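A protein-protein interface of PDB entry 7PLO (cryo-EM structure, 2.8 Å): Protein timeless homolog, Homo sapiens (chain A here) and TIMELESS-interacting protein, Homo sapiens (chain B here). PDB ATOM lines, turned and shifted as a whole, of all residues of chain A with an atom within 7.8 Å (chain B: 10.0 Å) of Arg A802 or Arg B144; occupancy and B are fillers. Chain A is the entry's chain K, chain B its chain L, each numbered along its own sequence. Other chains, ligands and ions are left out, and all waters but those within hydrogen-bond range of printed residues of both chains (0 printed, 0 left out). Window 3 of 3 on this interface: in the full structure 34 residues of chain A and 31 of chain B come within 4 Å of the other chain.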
ATOM      1  N   ALA A 741      30.361  -9.402   6.248  1.00  0.00           N
ATOM      2  CA  ALA A 741      29.733 -10.261   5.252  1.00  0.00           C
ATOM      3  C   ALA A 741      28.622 -11.112   5.848  1.00  0.00           C
ATOM      4  O   ALA A 741      27.717 -11.521   5.114  1.00  0.00           O
ATOM      5  CB  ALA A 741      30.775 -11.142   4.565  1.00  0.00           C
ATOM      6  N   LEU A 781      33.115  -4.040  -1.925  1.00  0.00           N
ATOM      7  CA  LEU A 781      33.267  -5.451  -2.276  1.00  0.00           C
ATOM      8  C   LEU A 781      32.570  -5.770  -3.593  1.00  0.00           C
ATOM      9  O   LEU A 781      33.046  -6.606  -4.366  1.00  0.00           O
ATOM     10  CB  LEU A 781      32.719  -6.343  -1.159  1.00  0.00           C
ATOM     11  CG  LEU A 781      32.712  -7.862  -1.405  1.00  0.00           C
ATOM     12  CD1 LEU A 781      34.116  -8.400  -1.661  1.00  0.00           C
ATOM     13  CD2 LEU A 781      32.074  -8.576  -0.235  1.00  0.00           C
ATOM     14  N   ASN A 785      33.996  -7.382  -6.927  1.00  0.00           N
ATOM     15  CA  ASN A 785      33.512  -8.719  -7.271  1.00  0.00           C
ATOM     16  C   ASN A 785      31.993  -8.699  -7.330  1.00  0.00           C
ATOM     17  O   ASN A 785      31.338  -8.415  -6.325  1.00  0.00           O
ATOM     18  CB  ASN A 785      34.006  -9.744  -6.243  1.00  0.00           C
ATOM     19  CG  ASN A 785      33.340 -11.102  -6.389  1.00  0.00           C
ATOM     20  OD1 ASN A 785      32.932 -11.502  -7.480  1.00  0.00           O
ATOM     21  ND2 ASN A 785      33.237 -11.825  -5.277  1.00  0.00           N
ATOM     22  N   LYS A 787      29.843 -11.167  -7.682  1.00  0.00           N
ATOM     23  CA  LYS A 787      29.114 -12.288  -7.092  1.00  0.00           C
ATOM     24  C   LYS A 787      28.558 -11.970  -5.702  1.00  0.00           C
ATOM     25  O   LYS A 787      27.745 -12.746  -5.179  1.00  0.00           O
ATOM     26  CB  LYS A 787      30.032 -13.516  -7.057  1.00  0.00           C
ATOM     27  CG  LYS A 787      30.418 -14.006  -8.460  1.00  0.00           C
ATOM     28  CD  LYS A 787      31.399 -15.178  -8.457  1.00  0.00           C
ATOM     29  CE  LYS A 787      32.811 -14.755  -8.069  1.00  0.00           C
ATOM     30  NZ  LYS A 787      33.826 -15.771  -8.475  1.00  0.00           N
ATOM     31  N   VAL A 790      24.785 -12.067  -5.618  1.00  0.00           N
ATOM     32  CA  VAL A 790      24.210 -13.383  -5.357  1.00  0.00           C
ATOM     33  C   VAL A 790      24.374 -13.745  -3.885  1.00  0.00           C
ATOM     34  O   VAL A 790      23.491 -14.370  -3.286  1.00  0.00           O
ATOM     35  CB  VAL A 790      24.840 -14.447  -6.277  1.00  0.00           C
ATOM     36  CG1 VAL A 790      24.430 -15.864  -5.834  1.00  0.00           C
ATOM     37  CG2 VAL A 790      24.454 -14.190  -7.741  1.00  0.00           C
ATOM     38  N   GLU A 791      25.509 -13.373  -3.284  1.00  0.00           N
ATOM     39  CA  GLU A 791      25.724 -13.687  -1.871  1.00  0.00           C
ATOM     40  C   GLU A 791      24.718 -13.002  -0.954  1.00  0.00           C
ATOM     41  O   GLU A 791      24.469 -13.499   0.151  1.00  0.00           O
ATOM     42  CB  GLU A 791      27.137 -13.297  -1.432  1.00  0.00           C
ATOM     43  CG  GLU A 791      28.256 -14.061  -2.119  1.00  0.00           C
ATOM     44  CD  GLU A 791      28.273 -15.536  -1.778  1.00  0.00           C
ATOM     45  OE1 GLU A 791      27.551 -15.952  -0.847  1.00  0.00           O
ATOM     46  OE2 GLU A 791      29.011 -16.288  -2.447  1.00  0.00           O
ATOM     47  N   PHE A 794      21.106 -15.163   0.579  1.00  0.00           N
ATOM     48  CA  PHE A 794      20.970 -16.245   1.553  1.00  0.00           C
ATOM     49  C   PHE A 794      21.790 -15.968   2.808  1.00  0.00           C
ATOM     50  O   PHE A 794      22.807 -15.270   2.766  1.00  0.00           O
ATOM     51  CB  PHE A 794      21.423 -17.592   0.973  1.00  0.00           C
ATOM     52  CG  PHE A 794      20.786 -17.937  -0.341  1.00  0.00           C
ATOM     53  CD1 PHE A 794      19.453 -18.300  -0.406  1.00  0.00           C
ATOM     54  CD2 PHE A 794      21.526 -17.913  -1.509  1.00  0.00           C
ATOM     55  CE1 PHE A 794      18.868 -18.624  -1.611  1.00  0.00           C
ATOM     56  CE2 PHE A 794      20.946 -18.235  -2.718  1.00  0.00           C
ATOM     57  CZ  PHE A 794      19.615 -18.591  -2.768  1.00  0.00           C
ATOM     58  N   LYS A 796      24.324 -17.487   5.765  1.00  0.00           N
ATOM     59  CA  LYS A 796      25.626 -18.090   5.465  1.00  0.00           C
ATOM     60  C   LYS A 796      26.320 -18.606   6.727  1.00  0.00           C
ATOM     61  O   LYS A 796      25.862 -18.371   7.849  1.00  0.00           O
ATOM     62  CB  LYS A 796      26.526 -17.073   4.762  1.00  0.00           C
ATOM     63  CG  LYS A 796      26.778 -15.807   5.582  1.00  0.00           C
ATOM     64  CD  LYS A 796      27.279 -14.669   4.724  1.00  0.00           C
ATOM     65  CE  LYS A 796      26.154 -14.012   3.939  1.00  0.00           C
ATOM     66  NZ  LYS A 796      26.651 -12.878   3.127  1.00  0.00           N
ATOM     67  N   ASN A 797      27.429 -19.348   6.523  1.00  0.00           N
ATOM     68  CA  ASN A 797      28.206 -19.939   7.619  1.00  0.00           C
ATOM     69  C   ASN A 797      29.664 -19.486   7.664  1.00  0.00           C
ATOM     70  O   ASN A 797      30.047 -18.749   8.575  1.00  0.00           O
ATOM     71  CB  ASN A 797      28.156 -21.462   7.481  1.00  0.00           C
ATOM     72  CG  ASN A 797      26.753 -22.004   7.424  1.00  0.00           C
ATOM     73  OD1 ASN A 797      25.798 -21.360   7.853  1.00  0.00           O
ATOM     74  ND2 ASN A 797      26.620 -23.214   6.891  1.00  0.00           N
ATOM     75  N   THR A 798      30.488 -19.900   6.688  1.00  0.00           N
ATOM     76  CA  THR A 798      31.898 -19.534   6.533  1.00  0.00           C
ATOM     77  C   THR A 798      32.137 -18.905   5.166  1.00  0.00           C
ATOM     78  O   THR A 798      33.269 -18.497   4.834  1.00  0.00           O
ATOM     79  CB  THR A 798      32.814 -20.759   6.693  1.00  0.00           C
ATOM     80  OG1 THR A 798      32.773 -21.543   5.494  1.00  0.00           O
ATOM     81  CG2 THR A 798      32.394 -21.633   7.879  1.00  0.00           C
ATOM     82  N   ALA A 799      31.075 -18.748   4.374  1.00  0.00           N
ATOM     83  CA  ALA A 799      31.150 -17.843   3.248  1.00  0.00           C
ATOM     84  C   ALA A 799      31.446 -16.413   3.689  1.00  0.00           C
ATOM     85  O   ALA A 799      31.921 -15.618   2.880  1.00  0.00           O
ATOM     86  CB  ALA A 799      29.859 -17.913   2.441  1.00  0.00           C
ATOM     87  N   VAL A 800      31.222 -16.086   4.968  1.00  0.00           N
ATOM     88  CA  VAL A 800      31.698 -14.843   5.570  1.00  0.00           C
ATOM     89  C   VAL A 800      33.198 -14.644   5.364  1.00  0.00           C
ATOM     90  O   VAL A 800      33.664 -13.503   5.365  1.00  0.00           O
ATOM     91  CB  VAL A 800      31.349 -14.801   7.080  1.00  0.00           C
ATOM     92  CG1 VAL A 800      31.789 -13.469   7.705  1.00  0.00           C
ATOM     93  CG2 VAL A 800      29.854 -15.032   7.336  1.00  0.00           C
ATOM     94  N   VAL A 801      33.981 -15.728   5.219  1.00  0.00           N
ATOM     95  CA  VAL A 801      35.414 -15.608   4.935  1.00  0.00           C
ATOM     96  C   VAL A 801      35.687 -15.838   3.452  1.00  0.00           C
ATOM     97  O   VAL A 801      36.630 -15.254   2.904  1.00  0.00           O
ATOM     98  CB  VAL A 801      36.281 -16.541   5.817  1.00  0.00           C
ATOM     99  CG1 VAL A 801      36.001 -16.277   7.288  1.00  0.00           C
ATOM    100  CG2 VAL A 801      36.131 -18.057   5.517  1.00  0.00           C
ATOM    101  N   ARG A 802      34.896 -16.698   2.790  1.00  0.00           N
ATOM    102  CA  ARG A 802      35.120 -16.882   1.347  1.00  0.00           C
ATOM    103  C   ARG A 802      34.887 -15.581   0.586  1.00  0.00           C
ATOM    104  O   ARG A 802      35.636 -15.256  -0.344  1.00  0.00           O
ATOM    105  CB  ARG A 802      34.228 -17.996   0.790  1.00  0.00           C
ATOM    106  CG  ARG A 802      34.005 -18.056  -0.736  1.00  0.00           C
ATOM    107  CD  ARG A 802      35.274 -18.268  -1.534  1.00  0.00           C
ATOM    108  NE  ARG A 802      34.969 -18.442  -2.952  1.00  0.00           N
ATOM    109  CZ  ARG A 802      34.748 -17.459  -3.820  1.00  0.00           C
ATOM    110  NH1 ARG A 802      34.824 -16.183  -3.470  1.00  0.00           N
ATOM    111  NH2 ARG A 802      34.437 -17.766  -5.076  1.00  0.00           N
ATOM    112  N   GLU A 803      33.834 -14.842   0.947  1.00  0.00           N
ATOM    113  CA  GLU A 803      33.611 -13.519   0.378  1.00  0.00           C
ATOM    114  C   GLU A 803      34.810 -12.615   0.624  1.00  0.00           C
ATOM    115  O   GLU A 803      35.194 -11.825  -0.246  1.00  0.00           O
ATOM    116  CB  GLU A 803      32.346 -12.899   0.977  1.00  0.00           C
ATOM    117  CG  GLU A 803      31.040 -13.572   0.562  1.00  0.00           C
ATOM    118  CD  GLU A 803      29.818 -12.815   1.045  1.00  0.00           C
ATOM    119  OE1 GLU A 803      29.785 -11.577   0.889  1.00  0.00           O
ATOM    120  OE2 GLU A 803      28.893 -13.455   1.589  1.00  0.00           O
ATOM    121  N   MET A 804      35.414 -12.720   1.804  1.00  0.00           N
ATOM    122  CA  MET A 804      36.638 -11.995   2.111  1.00  0.00           C
ATOM    123  C   MET A 804      37.830 -12.731   1.514  1.00  0.00           C
ATOM    124  O   MET A 804      37.669 -13.750   0.840  1.00  0.00           O
ATOM    125  CB  MET A 804      36.817 -11.840   3.623  1.00  0.00           C
ATOM    126  CG  MET A 804      35.660 -11.161   4.340  1.00  0.00           C
ATOM    127  SD  MET A 804      35.123  -9.568   3.680  1.00  0.00           S
ATOM    128  CE  MET A 804      33.845 -10.047   2.508  1.00  0.00           C
ATOM    129  N   LEU B  78      18.985 -17.599 -10.158  1.00  0.00           N
ATOM    130  CA  LEU B  78      20.404 -17.295  -9.973  1.00  0.00           C
ATOM    131  C   LEU B  78      21.210 -17.170 -11.267  1.00  0.00           C
ATOM    132  O   LEU B  78      22.089 -16.288 -11.318  1.00  0.00           O
ATOM    133  CB  LEU B  78      21.045 -18.351  -9.057  1.00  0.00           C
ATOM    134  CG  LEU B  78      20.831 -18.316  -7.530  1.00  0.00           C
ATOM    135  CD1 LEU B  78      21.116 -16.946  -6.911  1.00  0.00           C
ATOM    136  CD2 LEU B  78      19.438 -18.793  -7.144  1.00  0.00           C
ATOM    137  N   ARG B  82      23.132 -13.598 -11.891  1.00  0.00           N
ATOM    138  CA  ARG B  82      24.542 -13.397 -12.205  1.00  0.00           C
ATOM    139  C   ARG B  82      24.722 -12.282 -13.234  1.00  0.00           C
ATOM    140  O   ARG B  82      25.672 -11.496 -13.147  1.00  0.00           O
ATOM    141  CB  ARG B  82      25.145 -14.720 -12.696  1.00  0.00           C
ATOM    142  CG  ARG B  82      26.493 -14.651 -13.432  1.00  0.00           C
ATOM    143  CD  ARG B  82      27.611 -14.026 -12.608  1.00  0.00           C
ATOM    144  NE  ARG B  82      28.794 -13.792 -13.431  1.00  0.00           N
ATOM    145  CZ  ARG B  82      28.992 -12.738 -14.215  1.00  0.00           C
ATOM    146  NH1 ARG B  82      28.117 -11.745 -14.291  1.00  0.00           N
ATOM    147  NH2 ARG B  82      30.098 -12.678 -14.951  1.00  0.00           N
ATOM    148  N   GLY B 131      17.420 -21.284   0.808  1.00  0.00           N
ATOM    149  CA  GLY B 131      18.876 -21.337   0.875  1.00  0.00           C
ATOM    150  C   GLY B 131      19.452 -22.592   1.525  1.00  0.00           C
ATOM    151  O   GLY B 131      20.659 -22.829   1.390  1.00  0.00           O
ATOM    152  N   VAL B 136      20.044 -25.458  -4.372  1.00  0.00           N
ATOM    153  CA  VAL B 136      20.357 -24.042  -4.218  1.00  0.00           C
ATOM    154  C   VAL B 136      21.812 -23.862  -3.800  1.00  0.00           C
ATOM    155  O   VAL B 136      22.546 -23.071  -4.403  1.00  0.00           O
ATOM    156  CB  VAL B 136      19.383 -23.386  -3.219  1.00  0.00           C
ATOM    157  CG1 VAL B 136      19.694 -21.897  -3.039  1.00  0.00           C
ATOM    158  CG2 VAL B 136      17.925 -23.578  -3.682  1.00  0.00           C
ATOM    159  N   GLN B 137      22.265 -24.600  -2.777  1.00  0.00           N
ATOM    160  CA  GLN B 137      23.647 -24.388  -2.337  1.00  0.00           C
ATOM    161  C   GLN B 137      24.655 -24.965  -3.326  1.00  0.00           C
ATOM    162  O   GLN B 137      25.757 -24.418  -3.464  1.00  0.00           O
ATOM    163  CB  GLN B 137      23.896 -24.957  -0.936  1.00  0.00           C
ATOM    164  CG  GLN B 137      23.472 -26.408  -0.702  1.00  0.00           C
ATOM    165  CD  GLN B 137      22.382 -26.560   0.352  1.00  0.00           C
ATOM    166  OE1 GLN B 137      21.645 -25.622   0.650  1.00  0.00           O
ATOM    167  NE2 GLN B 137      22.262 -27.760   0.904  1.00  0.00           N
ATOM    168  N   THR B 138      24.312 -26.050  -4.028  1.00  0.00           N
ATOM    169  CA  THR B 138      25.207 -26.548  -5.068  1.00  0.00           C
ATOM    170  C   THR B 138      25.363 -25.528  -6.190  1.00  0.00           C
ATOM    171  O   THR B 138      26.480 -25.277  -6.661  1.00  0.00           O
ATOM    172  CB  THR B 138      24.697 -27.878  -5.625  1.00  0.00           C
ATOM    173  OG1 THR B 138      23.305 -27.771  -5.950  1.00  0.00           O
ATOM    174  CG2 THR B 138      24.914 -29.002  -4.615  1.00  0.00           C
ATOM    175  N   CYS B 139      24.256 -24.912  -6.620  1.00  0.00           N
ATOM    176  CA  CYS B 139      24.343 -23.864  -7.630  1.00  0.00           C
ATOM    177  C   CYS B 139      25.114 -22.660  -7.106  1.00  0.00           C
ATOM    178  O   CYS B 139      25.842 -22.006  -7.860  1.00  0.00           O
ATOM    179  CB  CYS B 139      22.943 -23.448  -8.078  1.00  0.00           C
ATOM    180  SG  CYS B 139      22.111 -24.655  -9.136  1.00  0.00           S
ATOM    181  N   LEU B 140      24.963 -22.349  -5.817  1.00  0.00           N
ATOM    182  CA  LEU B 140      25.690 -21.228  -5.230  1.00  0.00           C
ATOM    183  C   LEU B 140      27.195 -21.470  -5.273  1.00  0.00           C
ATOM    184  O   LEU B 140      27.968 -20.587  -5.667  1.00  0.00           O
ATOM    185  CB  LEU B 140      25.212 -21.002  -3.793  1.00  0.00           C
ATOM    186  CG  LEU B 140      25.814 -19.843  -2.993  1.00  0.00           C
ATOM    187  CD1 LEU B 140      25.552 -18.505  -3.663  1.00  0.00           C
ATOM    188  CD2 LEU B 140      25.253 -19.842  -1.577  1.00  0.00           C
ATOM    189  N   LYS B 141      27.630 -22.671  -4.885  1.00  0.00           N
ATOM    190  CA  LYS B 141      29.055 -22.989  -4.945  1.00  0.00           C
ATOM    191  C   LYS B 141      29.557 -23.019  -6.386  1.00  0.00           C
ATOM    192  O   LYS B 141      30.677 -22.574  -6.666  1.00  0.00           O
ATOM    193  CB  LYS B 141      29.332 -24.321  -4.245  1.00  0.00           C
ATOM    194  CG  LYS B 141      29.501 -24.194  -2.734  1.00  0.00           C
ATOM    195  CD  LYS B 141      29.956 -25.498  -2.090  1.00  0.00           C
ATOM    196  CE  LYS B 141      28.839 -26.528  -2.041  1.00  0.00           C
ATOM    197  NZ  LYS B 141      29.254 -27.762  -1.318  1.00  0.00           N
ATOM    198  N   ARG B 142      28.746 -23.535  -7.314  1.00  0.00           N
ATOM    199  CA  ARG B 142      29.147 -23.550  -8.719  1.00  0.00           C
ATOM    200  C   ARG B 142      29.330 -22.134  -9.259  1.00  0.00           C
ATOM    201  O   ARG B 142      30.304 -21.848  -9.974  1.00  0.00           O
ATOM    202  CB  ARG B 142      28.103 -24.310  -9.540  1.00  0.00           C
ATOM    203  CG  ARG B 142      28.436 -24.419 -11.015  1.00  0.00           C
ATOM    204  CD  ARG B 142      27.557 -25.434 -11.726  1.00  0.00           C
ATOM    205  NE  ARG B 142      27.872 -25.481 -13.150  1.00  0.00           N
ATOM    206  CZ  ARG B 142      27.500 -26.439 -13.991  1.00  0.00           C
ATOM    207  NH1 ARG B 142      26.791 -27.485 -13.592  1.00  0.00           N
ATOM    208  NH2 ARG B 142      27.857 -26.347 -15.269  1.00  0.00           N
ATOM    209  N   ILE B 143      28.402 -21.235  -8.922  1.00  0.00           N
ATOM    210  CA  ILE B 143      28.495 -19.845  -9.355  1.00  0.00           C
ATOM    211  C   ILE B 143      29.698 -19.173  -8.713  1.00  0.00           C
ATOM    212  O   ILE B 143      30.348 -18.318  -9.327  1.00  0.00           O
ATOM    213  CB  ILE B 143      27.180 -19.104  -9.038  1.00  0.00           C
ATOM    214  CG1 ILE B 143      26.077 -19.561 -10.000  1.00  0.00           C
ATOM    215  CG2 ILE B 143      27.364 -17.576  -9.113  1.00  0.00           C
ATOM    216  CD1 ILE B 143      24.663 -19.287  -9.519  1.00  0.00           C
ATOM    217  N   ARG B 144      30.002 -19.527  -7.462  1.00  0.00           N
ATOM    218  CA  ARG B 144      31.215 -19.015  -6.839  1.00  0.00           C
ATOM    219  C   ARG B 144      32.451 -19.481  -7.596  1.00  0.00           C
ATOM    220  O   ARG B 144      33.406 -18.713  -7.765  1.00  0.00           O
ATOM    221  CB  ARG B 144      31.299 -19.453  -5.372  1.00  0.00           C
ATOM    222  CG  ARG B 144      30.658 -18.482  -4.375  1.00  0.00           C
ATOM    223  CD  ARG B 144      31.148 -18.709  -2.941  1.00  0.00           C
ATOM    224  NE  ARG B 144      30.563 -19.892  -2.312  1.00  0.00           N
ATOM    225  CZ  ARG B 144      29.445 -19.919  -1.595  1.00  0.00           C
ATOM    226  NH1 ARG B 144      28.699 -18.838  -1.412  1.00  0.00           N
ATOM    227  NH2 ARG B 144      29.059 -21.065  -1.039  1.00  0.00           N
ATOM    228  N   LEU B 145      32.448 -20.728  -8.070  1.00  0.00           N
ATOM    229  CA  LEU B 145      33.673 -21.276  -8.653  1.00  0.00           C
ATOM    230  C   LEU B 145      33.876 -20.832 -10.101  1.00  0.00           C
ATOM    231  O   LEU B 145      34.781 -20.036 -10.375  1.00  0.00           O
ATOM    232  CB  LEU B 145      33.669 -22.805  -8.538  1.00  0.00           C
ATOM    233  CG  LEU B 145      34.455 -23.375  -7.350  1.00  0.00           C
ATOM    234  CD1 LEU B 145      34.027 -22.769  -6.010  1.00  0.00           C
ATOM    235  CD2 LEU B 145      34.313 -24.889  -7.307  1.00  0.00           C
ATOM    236  N   ASP B 146      33.055 -21.336 -11.043  1.00  0.00           N
ATOM    237  CA  ASP B 146      33.225 -20.948 -12.452  1.00  0.00           C
ATOM    238  C   ASP B 146      31.966 -20.480 -13.180  1.00  0.00           C
ATOM    239  O   ASP B 146      31.865 -19.301 -13.534  1.00  0.00           O
ATOM    240  CB  ASP B 146      33.859 -22.111 -13.222  1.00  0.00           C
ATOM    241  CG  ASP B 146      33.289 -23.461 -12.827  1.00  0.00           C
ATOM    242  OD1 ASP B 146      32.379 -23.497 -11.973  1.00  0.00           O
ATOM    243  OD2 ASP B 146      33.754 -24.484 -13.372  1.00  0.00           O
ATOM    244  N   LEU B 147      30.988 -21.369 -13.357  1.00  0.00           N
ATOM    245  CA  LEU B 147      29.778 -21.099 -14.152  1.00  0.00           C
ATOM    246  C   LEU B 147      28.913 -22.354 -14.182  1.00  0.00           C
ATOM    247  O   LEU B 147      29.424 -23.465 -14.331  1.00  0.00           O
ATOM    248  CB  LEU B 147      30.090 -20.655 -15.606  1.00  0.00           C
ATOM    249  CG  LEU B 147      30.596 -21.627 -16.685  1.00  0.00           C
ATOM    250  CD1 LEU B 147      30.560 -20.948 -18.054  1.00  0.00           C
ATOM    251  CD2 LEU B 147      31.997 -22.118 -16.394  1.00  0.00           C
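NZ of Lys A787 lies within hydrogen-bond range of O of Arg B144 (3.1 Å). The guanidinium group of Arg A802 lies within hydrogen-bond range of the backbone carbonyl oxygen of Arg B144 (3.0 Å). The guanidinium group of Arg B144 is in salt-bridge range of the side-chain carboxylate of Glu A791 (2.8 Å).
N of Lys A787 sits at hydrogen-bond distance from OD1 of Asn A785. OE1 of Gln B137 lies close to O of Gly B131, 3.1 Å away.
Among the printed residues, merely in contact across the chains: Lys A787 with Ile B143 (3.4 Å), Val A790 with Leu B78 (3.6 Å), Val A790 with Leu B140 (3.6 Å), Phe A794 with Gly B131 (3.3 Å) and Phe A794 with Val B136 (3.3 Å).
Leu A781 touches none of the printed residues of chain B. Printed residues of chain B within 4 Å of Lys A787: Ile B143 (3.4 Å) and Arg B144 (3.1 Å). Of the printed residues of chain B, Glu A791 touches Arg B144. No residue of chain B comes within 4 Å of Ala A799. No residue of chain B comes within 4 Å of Val A801. Of the printed residues of chain B, Arg A802 touches Arg B144. Of the printed residues of chain A, Gly B131 touches Phe A794. Printed residues of chain A within 4 Å of Ile B143: Lys A787 (3.4 Å). The nearest residue of chain A that does not touch Arg B144 is Ala A799 (4.1 Å).
Of the 15 printed residues of chain B, 6 touch a printed residue of chain A. Hydrophobic or aromatic side chains of chain B within 4 Å of the printed part of chain A: Leu B78, Val B136 and Leu B140. Hydrophobic or aromatic side chains of chain A that line the printed part of chain B: Val A790 and Phe A794.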
